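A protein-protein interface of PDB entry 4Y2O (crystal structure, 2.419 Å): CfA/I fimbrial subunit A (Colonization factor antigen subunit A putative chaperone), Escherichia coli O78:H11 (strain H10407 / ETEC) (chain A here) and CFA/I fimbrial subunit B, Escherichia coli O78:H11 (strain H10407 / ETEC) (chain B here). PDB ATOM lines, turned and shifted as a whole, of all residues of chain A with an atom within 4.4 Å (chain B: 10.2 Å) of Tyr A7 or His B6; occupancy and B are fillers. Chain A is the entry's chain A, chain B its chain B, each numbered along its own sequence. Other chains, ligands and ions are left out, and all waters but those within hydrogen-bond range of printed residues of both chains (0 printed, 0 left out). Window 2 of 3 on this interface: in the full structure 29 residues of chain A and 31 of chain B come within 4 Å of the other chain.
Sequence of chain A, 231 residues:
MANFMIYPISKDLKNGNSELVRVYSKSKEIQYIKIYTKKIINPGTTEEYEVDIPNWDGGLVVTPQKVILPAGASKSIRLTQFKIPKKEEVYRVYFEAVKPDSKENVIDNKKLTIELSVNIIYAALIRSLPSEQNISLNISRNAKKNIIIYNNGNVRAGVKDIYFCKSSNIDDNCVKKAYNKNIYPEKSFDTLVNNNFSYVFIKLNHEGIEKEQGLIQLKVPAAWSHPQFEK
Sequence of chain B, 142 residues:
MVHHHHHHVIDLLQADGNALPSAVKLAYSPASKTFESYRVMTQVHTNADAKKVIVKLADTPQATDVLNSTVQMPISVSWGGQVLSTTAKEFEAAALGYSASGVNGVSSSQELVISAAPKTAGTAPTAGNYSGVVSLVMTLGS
The backbone carbonyl oxygen (O) of Tyr A7 lies within hydrogen-bond range of the backbone NH (N) of Arg A22.
The side-chain hydroxyl of Tyr A7 is in hydrogen-bond range of a ring nitrogen (ND1) of His B6 (3.1 Å).
Of chain B, only His B6 (3.1 Å) and Val B9 (3.5 Å) come within 4 Å of Tyr A7.
Ile A6 touches just one residue of chain B: Val B9 (3.8 Å).
Pro A8 touches two residues of chain B.
Of the printed residues of chain A, Val B9 touches Ile A6 (3.8 Å) and Tyr A7 (3.5 Å).
Printed residues of chain B within 4 Å of Lys A11: His B6 (3.6 Å).
Of the printed residues of chain A, His B8 touches Pro A8.
The nearest residue of chain B that does not touch Tyr A7 is His B8 (4.5 Å).
The nearest printed residue of chain A that does not touch Val B9 is Pro A8 (5.2 Å).
Printed residues of chain B that touch a printed residue of chain A: His B6, His B8 and Val B9.
Hydrophobic or aromatic side chains of chain B within 4 Å of the printed part of chain A: His B6 and Val B9.
Along chain B the printed residues that touch a printed residue of chain A span positions 6 to 9.
Of the 8 printed residues of chain A, 4 touch a printed residue of chain B.
Printed residues of chain A that touch a printed residue of chain B: Ile A6, Tyr A7, Pro A8 and Lys A11.
Hydrophobic or aromatic side chains of chain A that line the printed part of chain B: Tyr A7 and Pro A8.
Among the printed residues, pairs that only touch across the chains: Ile A6 with Val B9, Tyr A7 with Val B9, Pro A8 with His B6, Pro A8 with His B8 and Lys A11 with His B6.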
ATOM      1  N   ILE A   6     -10.129 -18.919  33.289  1.00  0.00           N
ATOM      2  CA  ILE A   6     -11.173 -18.831  32.304  1.00  0.00           C
ATOM      3  C   ILE A   6     -10.686 -18.309  30.980  1.00  0.00           C
ATOM      4  O   ILE A   6      -9.756 -17.539  30.907  1.00  0.00           O
ATOM      5  CB  ILE A   6     -12.332 -17.945  32.766  1.00  0.00           C
ATOM      6  CG1 ILE A   6     -11.919 -16.487  32.850  1.00  0.00           C
ATOM      7  CG2 ILE A   6     -12.870 -18.428  34.066  1.00  0.00           C
ATOM      8  CD1 ILE A   6     -13.053 -15.561  32.800  1.00  0.00           C
ATOM      9  N   TYR A   7     -11.344 -18.751  29.925  1.00  0.00           N
ATOM     10  CA  TYR A   7     -11.065 -18.260  28.605  1.00  0.00           C
ATOM     11  C   TYR A   7     -12.331 -18.045  27.813  1.00  0.00           C
ATOM     12  O   TYR A   7     -13.168 -18.916  27.733  1.00  0.00           O
ATOM     13  CB  TYR A   7     -10.152 -19.221  27.860  1.00  0.00           C
ATOM     14  CG  TYR A   7      -9.792 -18.739  26.487  1.00  0.00           C
ATOM     15  CD1 TYR A   7     -10.597 -19.012  25.406  1.00  0.00           C
ATOM     16  CD2 TYR A   7      -8.663 -17.998  26.278  1.00  0.00           C
ATOM     17  CE1 TYR A   7     -10.289 -18.568  24.182  1.00  0.00           C
ATOM     18  CE2 TYR A   7      -8.350 -17.551  25.051  1.00  0.00           C
ATOM     19  CZ  TYR A   7      -9.161 -17.844  24.003  1.00  0.00           C
ATOM     20  OH  TYR A   7      -8.848 -17.401  22.759  1.00  0.00           O
ATOM     21  N   PRO A   8     -12.464 -16.875  27.204  1.00  0.00           N
ATOM     22  CA  PRO A   8     -11.601 -15.712  27.326  1.00  0.00           C
ATOM     23  C   PRO A   8     -12.098 -14.765  28.389  1.00  0.00           C
ATOM     24  O   PRO A   8     -13.022 -15.096  29.100  1.00  0.00           O
ATOM     25  CB  PRO A   8     -11.709 -15.077  25.960  1.00  0.00           C
ATOM     26  CG  PRO A   8     -13.048 -15.368  25.562  1.00  0.00           C
ATOM     27  CD  PRO A   8     -13.374 -16.725  26.069  1.00  0.00           C
ATOM     28  N   LYS A  11     -15.500 -10.537  25.633  1.00  0.00           N
ATOM     29  CA  LYS A  11     -16.326 -11.121  24.604  1.00  0.00           C
ATOM     30  C   LYS A  11     -17.309 -10.135  24.031  1.00  0.00           C
ATOM     31  O   LYS A  11     -17.804  -9.275  24.725  1.00  0.00           O
ATOM     32  CB  LYS A  11     -17.086 -12.319  25.145  1.00  0.00           C
ATOM     33  CG  LYS A  11     -16.724 -13.625  24.508  1.00  0.00           C
ATOM     34  CD  LYS A  11     -16.550 -13.477  23.030  1.00  0.00           C
ATOM     35  CE  LYS A  11     -16.118 -14.771  22.393  1.00  0.00           C
ATOM     36  NZ  LYS A  11     -15.952 -14.598  20.926  1.00  0.00           N
ATOM     37  N   LEU A  20     -19.281 -18.795  24.320  1.00  0.00           N
ATOM     38  CA  LEU A  20     -18.915 -19.593  25.473  1.00  0.00           C
ATOM     39  C   LEU A  20     -17.707 -19.051  26.204  1.00  0.00           C
ATOM     40  O   LEU A  20     -16.761 -18.605  25.588  1.00  0.00           O
ATOM     41  CB  LEU A  20     -18.638 -21.019  25.047  1.00  0.00           C
ATOM     42  CG  LEU A  20     -19.788 -21.722  24.360  1.00  0.00           C
ATOM     43  CD1 LEU A  20     -19.318 -23.040  23.899  1.00  0.00           C
ATOM     44  CD2 LEU A  20     -20.928 -21.896  25.296  1.00  0.00           C
ATOM     45  N   VAL A  21     -17.753 -19.084  27.523  1.00  0.00           N
ATOM     46  CA  VAL A  21     -16.572 -18.875  28.321  1.00  0.00           C
ATOM     47  C   VAL A  21     -16.194 -20.192  28.933  1.00  0.00           C
ATOM     48  O   VAL A  21     -17.014 -20.853  29.527  1.00  0.00           O
ATOM     49  CB  VAL A  21     -16.778 -17.850  29.414  1.00  0.00           C
ATOM     50  CG1 VAL A  21     -15.699 -17.965  30.416  1.00  0.00           C
ATOM     51  CG2 VAL A  21     -16.759 -16.491  28.841  1.00  0.00           C
ATOM     52  N   ARG A  22     -14.950 -20.590  28.776  1.00  0.00           N
ATOM     53  CA  ARG A  22     -14.546 -21.868  29.302  1.00  0.00           C
ATOM     54  C   ARG A  22     -13.772 -21.709  30.580  1.00  0.00           C
ATOM     55  O   ARG A  22     -12.981 -20.807  30.726  1.00  0.00           O
ATOM     56  CB  ARG A  22     -13.737 -22.636  28.268  1.00  0.00           C
ATOM     57  CG  ARG A  22     -14.585 -23.227  27.185  1.00  0.00           C
ATOM     58  CD  ARG A  22     -13.770 -23.697  26.014  1.00  0.00           C
ATOM     59  NE  ARG A  22     -14.589 -24.351  25.005  1.00  0.00           N
ATOM     60  CZ  ARG A  22     -14.957 -23.793  23.860  1.00  0.00           C
ATOM     61  NH1 ARG A  22     -14.580 -22.569  23.559  1.00  0.00           N
ATOM     62  NH2 ARG A  22     -15.702 -24.467  23.014  1.00  0.00           N
ATOM     63  N   TYR A  24     -11.328 -23.560  33.409  1.00  0.00           N
ATOM     64  CA  TYR A  24     -10.411 -24.659  33.584  1.00  0.00           C
ATOM     65  C   TYR A  24      -9.863 -24.702  34.982  1.00  0.00           C
ATOM     66  O   TYR A  24      -9.390 -23.720  35.487  1.00  0.00           O
ATOM     67  CB  TYR A  24      -9.258 -24.572  32.596  1.00  0.00           C
ATOM     68  CG  TYR A  24      -9.652 -24.451  31.160  1.00  0.00           C
ATOM     69  CD1 TYR A  24      -9.995 -23.241  30.622  1.00  0.00           C
ATOM     70  CD2 TYR A  24      -9.654 -25.539  30.338  1.00  0.00           C
ATOM     71  CE1 TYR A  24     -10.342 -23.128  29.323  1.00  0.00           C
ATOM     72  CE2 TYR A  24     -10.001 -25.435  29.040  1.00  0.00           C
ATOM     73  CZ  TYR A  24     -10.341 -24.229  28.533  1.00  0.00           C
ATOM     74  OH  TYR A  24     -10.691 -24.118  27.228  1.00  0.00           O
ATOM     75  N   MET B   1      -3.136 -18.378  12.316  1.00  0.00           N
ATOM     76  CA  MET B   1      -3.965 -19.118  11.381  1.00  0.00           C
ATOM     77  C   MET B   1      -5.375 -18.569  11.310  1.00  0.00           C
ATOM     78  O   MET B   1      -5.607 -17.387  11.535  1.00  0.00           O
ATOM     79  CB  MET B   1      -4.005 -20.588  11.772  1.00  0.00           C
ATOM     80  CG  MET B   1      -3.443 -20.853  13.145  1.00  0.00           C
ATOM     81  SD  MET B   1      -1.742 -21.390  13.066  1.00  0.00           S
ATOM     82  CE  MET B   1      -1.935 -22.868  12.082  1.00  0.00           C
ATOM     83  N   VAL B   2      -6.317 -19.442  10.983  1.00  0.00           N
ATOM     84  CA  VAL B   2      -7.718 -19.058  10.923  1.00  0.00           C
ATOM     85  C   VAL B   2      -8.252 -18.771  12.316  1.00  0.00           C
ATOM     86  O   VAL B   2      -8.089 -19.582  13.227  1.00  0.00           O
ATOM     87  CB  VAL B   2      -8.577 -20.146  10.259  1.00  0.00           C
ATOM     88  CG1 VAL B   2      -8.474 -20.050   8.745  1.00  0.00           C
ATOM     89  CG2 VAL B   2      -8.165 -21.526  10.749  1.00  0.00           C
ATOM     90  N   HIS B   3      -8.886 -17.613  12.469  1.00  0.00           N
ATOM     91  CA  HIS B   3      -9.356 -17.178  13.769  1.00  0.00           C
ATOM     92  C   HIS B   3     -10.255 -18.236  14.408  1.00  0.00           C
ATOM     93  O   HIS B   3     -11.030 -18.853  13.681  1.00  0.00           O
ATOM     94  CB  HIS B   3     -10.085 -15.836  13.680  1.00  0.00           C
ATOM     95  CG  HIS B   3     -10.594 -15.495  12.320  1.00  0.00           C
ATOM     96  ND1 HIS B   3     -11.442 -16.316  11.613  1.00  0.00           N
ATOM     97  CD2 HIS B   3     -10.402 -14.398  11.554  1.00  0.00           C
ATOM     98  CE1 HIS B   3     -11.738 -15.746  10.460  1.00  0.00           C
ATOM     99  NE2 HIS B   3     -11.120 -14.582  10.399  1.00  0.00           N
ATOM    100  N   HIS B   4     -10.175 -18.485  15.729  1.00  0.00           N
ATOM    101  CA  HIS B   4      -9.346 -17.802  16.745  1.00  0.00           C
ATOM    102  C   HIS B   4      -9.816 -16.361  16.845  1.00  0.00           C
ATOM    103  O   HIS B   4      -9.060 -15.420  16.648  1.00  0.00           O
ATOM    104  CB  HIS B   4      -7.844 -17.956  16.422  1.00  0.00           C
ATOM    105  CG  HIS B   4      -6.916 -17.129  17.255  1.00  0.00           C
ATOM    106  ND1 HIS B   4      -6.975 -15.756  17.299  1.00  0.00           N
ATOM    107  CD2 HIS B   4      -5.842 -17.480  17.998  1.00  0.00           C
ATOM    108  CE1 HIS B   4      -6.011 -15.303  18.079  1.00  0.00           C
ATOM    109  NE2 HIS B   4      -5.308 -16.329  18.515  1.00  0.00           N
ATOM    110  N   HIS B   5     -11.107 -16.220  17.117  1.00  0.00           N
ATOM    111  CA  HIS B   5     -11.758 -14.926  17.190  1.00  0.00           C
ATOM    112  C   HIS B   5     -11.236 -14.152  18.345  1.00  0.00           C
ATOM    113  O   HIS B   5     -10.649 -13.089  18.180  1.00  0.00           O
ATOM    114  CB  HIS B   5     -13.258 -15.065  17.365  1.00  0.00           C
ATOM    115  CG  HIS B   5     -13.891 -16.024  16.415  1.00  0.00           C
ATOM    116  ND1 HIS B   5     -15.230 -16.334  16.462  1.00  0.00           N
ATOM    117  CD2 HIS B   5     -13.375 -16.740  15.392  1.00  0.00           C
ATOM    118  CE1 HIS B   5     -15.515 -17.197  15.507  1.00  0.00           C
ATOM    119  NE2 HIS B   5     -14.405 -17.463  14.845  1.00  0.00           N
ATOM    120  N   HIS B   6     -11.475 -14.693  19.533  1.00  0.00           N
ATOM    121  CA  HIS B   6     -11.193 -13.980  20.767  1.00  0.00           C
ATOM    122  C   HIS B   6      -9.692 -13.982  21.013  1.00  0.00           C
ATOM    123  O   HIS B   6      -9.011 -14.939  20.673  1.00  0.00           O
ATOM    124  CB  HIS B   6     -11.956 -14.602  21.944  1.00  0.00           C
ATOM    125  CG  HIS B   6     -12.191 -16.081  21.826  1.00  0.00           C
ATOM    126  ND1 HIS B   6     -11.393 -16.915  21.070  1.00  0.00           N
ATOM    127  CD2 HIS B   6     -13.143 -16.873  22.371  1.00  0.00           C
ATOM    128  CE1 HIS B   6     -11.842 -18.154  21.158  1.00  0.00           C
ATOM    129  NE2 HIS B   6     -12.902 -18.156  21.944  1.00  0.00           N
ATOM    130  N   HIS B   7      -9.176 -12.906  21.596  1.00  0.00           N
ATOM    131  CA  HIS B   7      -7.753 -12.869  21.853  1.00  0.00           C
ATOM    132  C   HIS B   7      -7.277 -12.523  23.278  1.00  0.00           C
ATOM    133  O   HIS B   7      -6.102 -12.256  23.457  1.00  0.00           O
ATOM    134  CB  HIS B   7      -7.059 -11.976  20.782  1.00  0.00           C
ATOM    135  CG  HIS B   7      -7.329 -10.498  20.862  1.00  0.00           C
ATOM    136  ND1 HIS B   7      -6.571  -9.584  20.161  1.00  0.00           N
ATOM    137  CD2 HIS B   7      -8.262  -9.773  21.524  1.00  0.00           C
ATOM    138  CE1 HIS B   7      -7.013  -8.365  20.395  1.00  0.00           C
ATOM    139  NE2 HIS B   7      -8.038  -8.448  21.221  1.00  0.00           N
ATOM    140  N   HIS B   8      -8.143 -12.520  24.287  1.00  0.00           N
ATOM    141  CA  HIS B   8      -7.739 -12.010  25.606  1.00  0.00           C
ATOM    142  C   HIS B   8      -7.891 -12.990  26.760  1.00  0.00           C
ATOM    143  O   HIS B   8      -8.953 -13.516  27.008  1.00  0.00           O
ATOM    144  CB  HIS B   8      -8.504 -10.755  25.961  1.00  0.00           C
ATOM    145  CG  HIS B   8      -8.101  -9.559  25.170  1.00  0.00           C
ATOM    146  ND1 HIS B   8      -6.789  -9.179  25.016  1.00  0.00           N
ATOM    147  CD2 HIS B   8      -8.837  -8.649  24.502  1.00  0.00           C
ATOM    148  CE1 HIS B   8      -6.735  -8.086  24.281  1.00  0.00           C
ATOM    149  NE2 HIS B   8      -7.965  -7.742  23.957  1.00  0.00           N
ATOM    150  N   VAL B   9      -6.792 -13.213  27.463  1.00  0.00           N
ATOM    151  CA  VAL B   9      -6.735 -14.133  28.586  1.00  0.00           C
ATOM    152  C   VAL B   9      -5.985 -13.550  29.755  1.00  0.00           C
ATOM    153  O   VAL B   9      -5.141 -12.700  29.585  1.00  0.00           O
ATOM    154  CB  VAL B   9      -6.030 -15.434  28.235  1.00  0.00           C
ATOM    155  CG1 VAL B   9      -6.692 -16.590  28.928  1.00  0.00           C
ATOM    156  CG2 VAL B   9      -6.028 -15.653  26.768  1.00  0.00           C
ATOM    157  N   ILE B  10      -6.285 -14.041  30.945  1.00  0.00           N
ATOM    158  CA  ILE B  10      -5.551 -13.682  32.139  1.00  0.00           C
ATOM    159  C   ILE B  10      -5.360 -14.898  33.011  1.00  0.00           C
ATOM    160  O   ILE B  10      -6.324 -15.551  33.365  1.00  0.00           O
ATOM    161  CB  ILE B  10      -6.277 -12.627  32.963  1.00  0.00           C
ATOM    162  CG1 ILE B  10      -6.211 -11.272  32.291  1.00  0.00           C
ATOM    163  CG2 ILE B  10      -5.662 -12.521  34.318  1.00  0.00           C
ATOM    164  CD1 ILE B  10      -6.917 -10.215  33.051  1.00  0.00           C
ATOM    165  N   ASP B  11      -4.124 -15.208  33.362  1.00  0.00           N
ATOM    166  CA  ASP B  11      -3.894 -16.217  34.370  1.00  0.00           C
ATOM    167  C   ASP B  11      -2.784 -15.774  35.284  1.00  0.00           C
ATOM    168  O   ASP B  11      -1.685 -15.495  34.839  1.00  0.00           O
ATOM    169  CB  ASP B  11      -3.560 -17.554  33.734  1.00  0.00           C
ATOM    170  CG  ASP B  11      -3.705 -18.702  34.695  1.00  0.00           C
ATOM    171  OD1 ASP B  11      -4.331 -18.513  35.747  1.00  0.00           O
ATOM    172  OD2 ASP B  11      -3.199 -19.796  34.392  1.00  0.00           O
ATOM    173  N   HIS B  45      -0.095 -14.488  33.138  1.00  0.00           N
ATOM    174  CA  HIS B  45      -0.088 -15.068  31.815  1.00  0.00           C
ATOM    175  C   HIS B  45      -1.214 -14.551  30.947  1.00  0.00           C
ATOM    176  O   HIS B  45      -2.374 -14.758  31.248  1.00  0.00           O
ATOM    177  CB  HIS B  45      -0.142 -16.580  31.929  1.00  0.00           C
ATOM    178  CG  HIS B  45       1.209 -17.209  31.987  1.00  0.00           C
ATOM    179  ND1 HIS B  45       1.575 -18.277  31.196  1.00  0.00           N
ATOM    180  CD2 HIS B  45       2.304 -16.888  32.714  1.00  0.00           C
ATOM    181  CE1 HIS B  45       2.832 -18.597  31.449  1.00  0.00           C
ATOM    182  NE2 HIS B  45       3.297 -17.771  32.367  1.00  0.00           N
ATOM    183  N   THR B  46      -0.845 -13.869  29.869  1.00  0.00           N
ATOM    184  CA  THR B  46      -1.774 -13.120  29.037  1.00  0.00           C
ATOM    185  C   THR B  46      -1.314 -13.035  27.606  1.00  0.00           C
ATOM    186  O   THR B  46      -0.139 -12.955  27.352  1.00  0.00           O
ATOM    187  CB  THR B  46      -1.914 -11.704  29.504  1.00  0.00           C
ATOM    188  OG1 THR B  46      -0.618 -11.117  29.549  1.00  0.00           O
ATOM    189  CG2 THR B  46      -2.516 -11.618  30.868  1.00  0.00           C
ATOM    190  N   ASN B  47      -2.244 -12.989  26.670  1.00  0.00           N
ATOM    191  CA  ASN B  47      -1.902 -12.669  25.297  1.00  0.00           C
ATOM    192  C   ASN B  47      -1.522 -11.210  25.146  1.00  0.00           C
ATOM    193  O   ASN B  47      -1.959 -10.373  25.926  1.00  0.00           O
ATOM    194  CB  ASN B  47      -3.066 -12.968  24.372  1.00  0.00           C
ATOM    195  CG  ASN B  47      -3.272 -14.422  24.169  1.00  0.00           C
ATOM    196  OD1 ASN B  47      -2.323 -15.191  24.145  1.00  0.00           O
ATOM    197  ND2 ASN B  47      -4.517 -14.820  24.007  1.00  0.00           N
ATOM    198  N   ALA B  48      -0.735 -10.913  24.120  1.00  0.00           N
ATOM    199  CA  ALA B  48      -0.398  -9.545  23.767  1.00  0.00           C
ATOM    200  C   ALA B  48      -1.635  -8.667  23.686  1.00  0.00           C
ATOM    201  O   ALA B  48      -2.701  -9.125  23.302  1.00  0.00           O
ATOM    202  CB  ALA B  48       0.344  -9.517  22.467  1.00  0.00           C
ATOM    203  N   ASP B  49      -1.449  -7.402  24.041  1.00  0.00           N
ATOM    204  CA  ASP B  49      -2.503  -6.415  24.309  1.00  0.00           C
ATOM    205  C   ASP B  49      -3.050  -6.632  25.693  1.00  0.00           C
ATOM    206  O   ASP B  49      -4.007  -5.986  26.104  1.00  0.00           O
ATOM    207  CB  ASP B  49      -3.646  -6.452  23.306  1.00  0.00           C
ATOM    208  CG  ASP B  49      -4.485  -5.190  23.346  1.00  0.00           C
ATOM    209  OD1 ASP B  49      -4.117  -4.224  22.654  1.00  0.00           O
ATOM    210  OD2 ASP B  49      -5.497  -5.149  24.072  1.00  0.00           O
ATOM    211  N   LEU B 140     -10.579  -6.692  32.906  1.00  0.00           N
ATOM    212  CA  LEU B 140     -10.125  -5.679  32.000  1.00  0.00           C
ATOM    213  C   LEU B 140     -10.955  -4.453  32.211  1.00  0.00           C
ATOM    214  O   LEU B 140     -11.942  -4.474  32.922  1.00  0.00           O
ATOM    215  CB  LEU B 140     -10.228  -6.128  30.556  1.00  0.00           C
ATOM    216  CG  LEU B 140      -9.410  -7.330  30.121  1.00  0.00           C
ATOM    217  CD1 LEU B 140      -9.429  -7.426  28.634  1.00  0.00           C
ATOM    218  CD2 LEU B 140      -8.004  -7.242  30.626  1.00  0.00           C
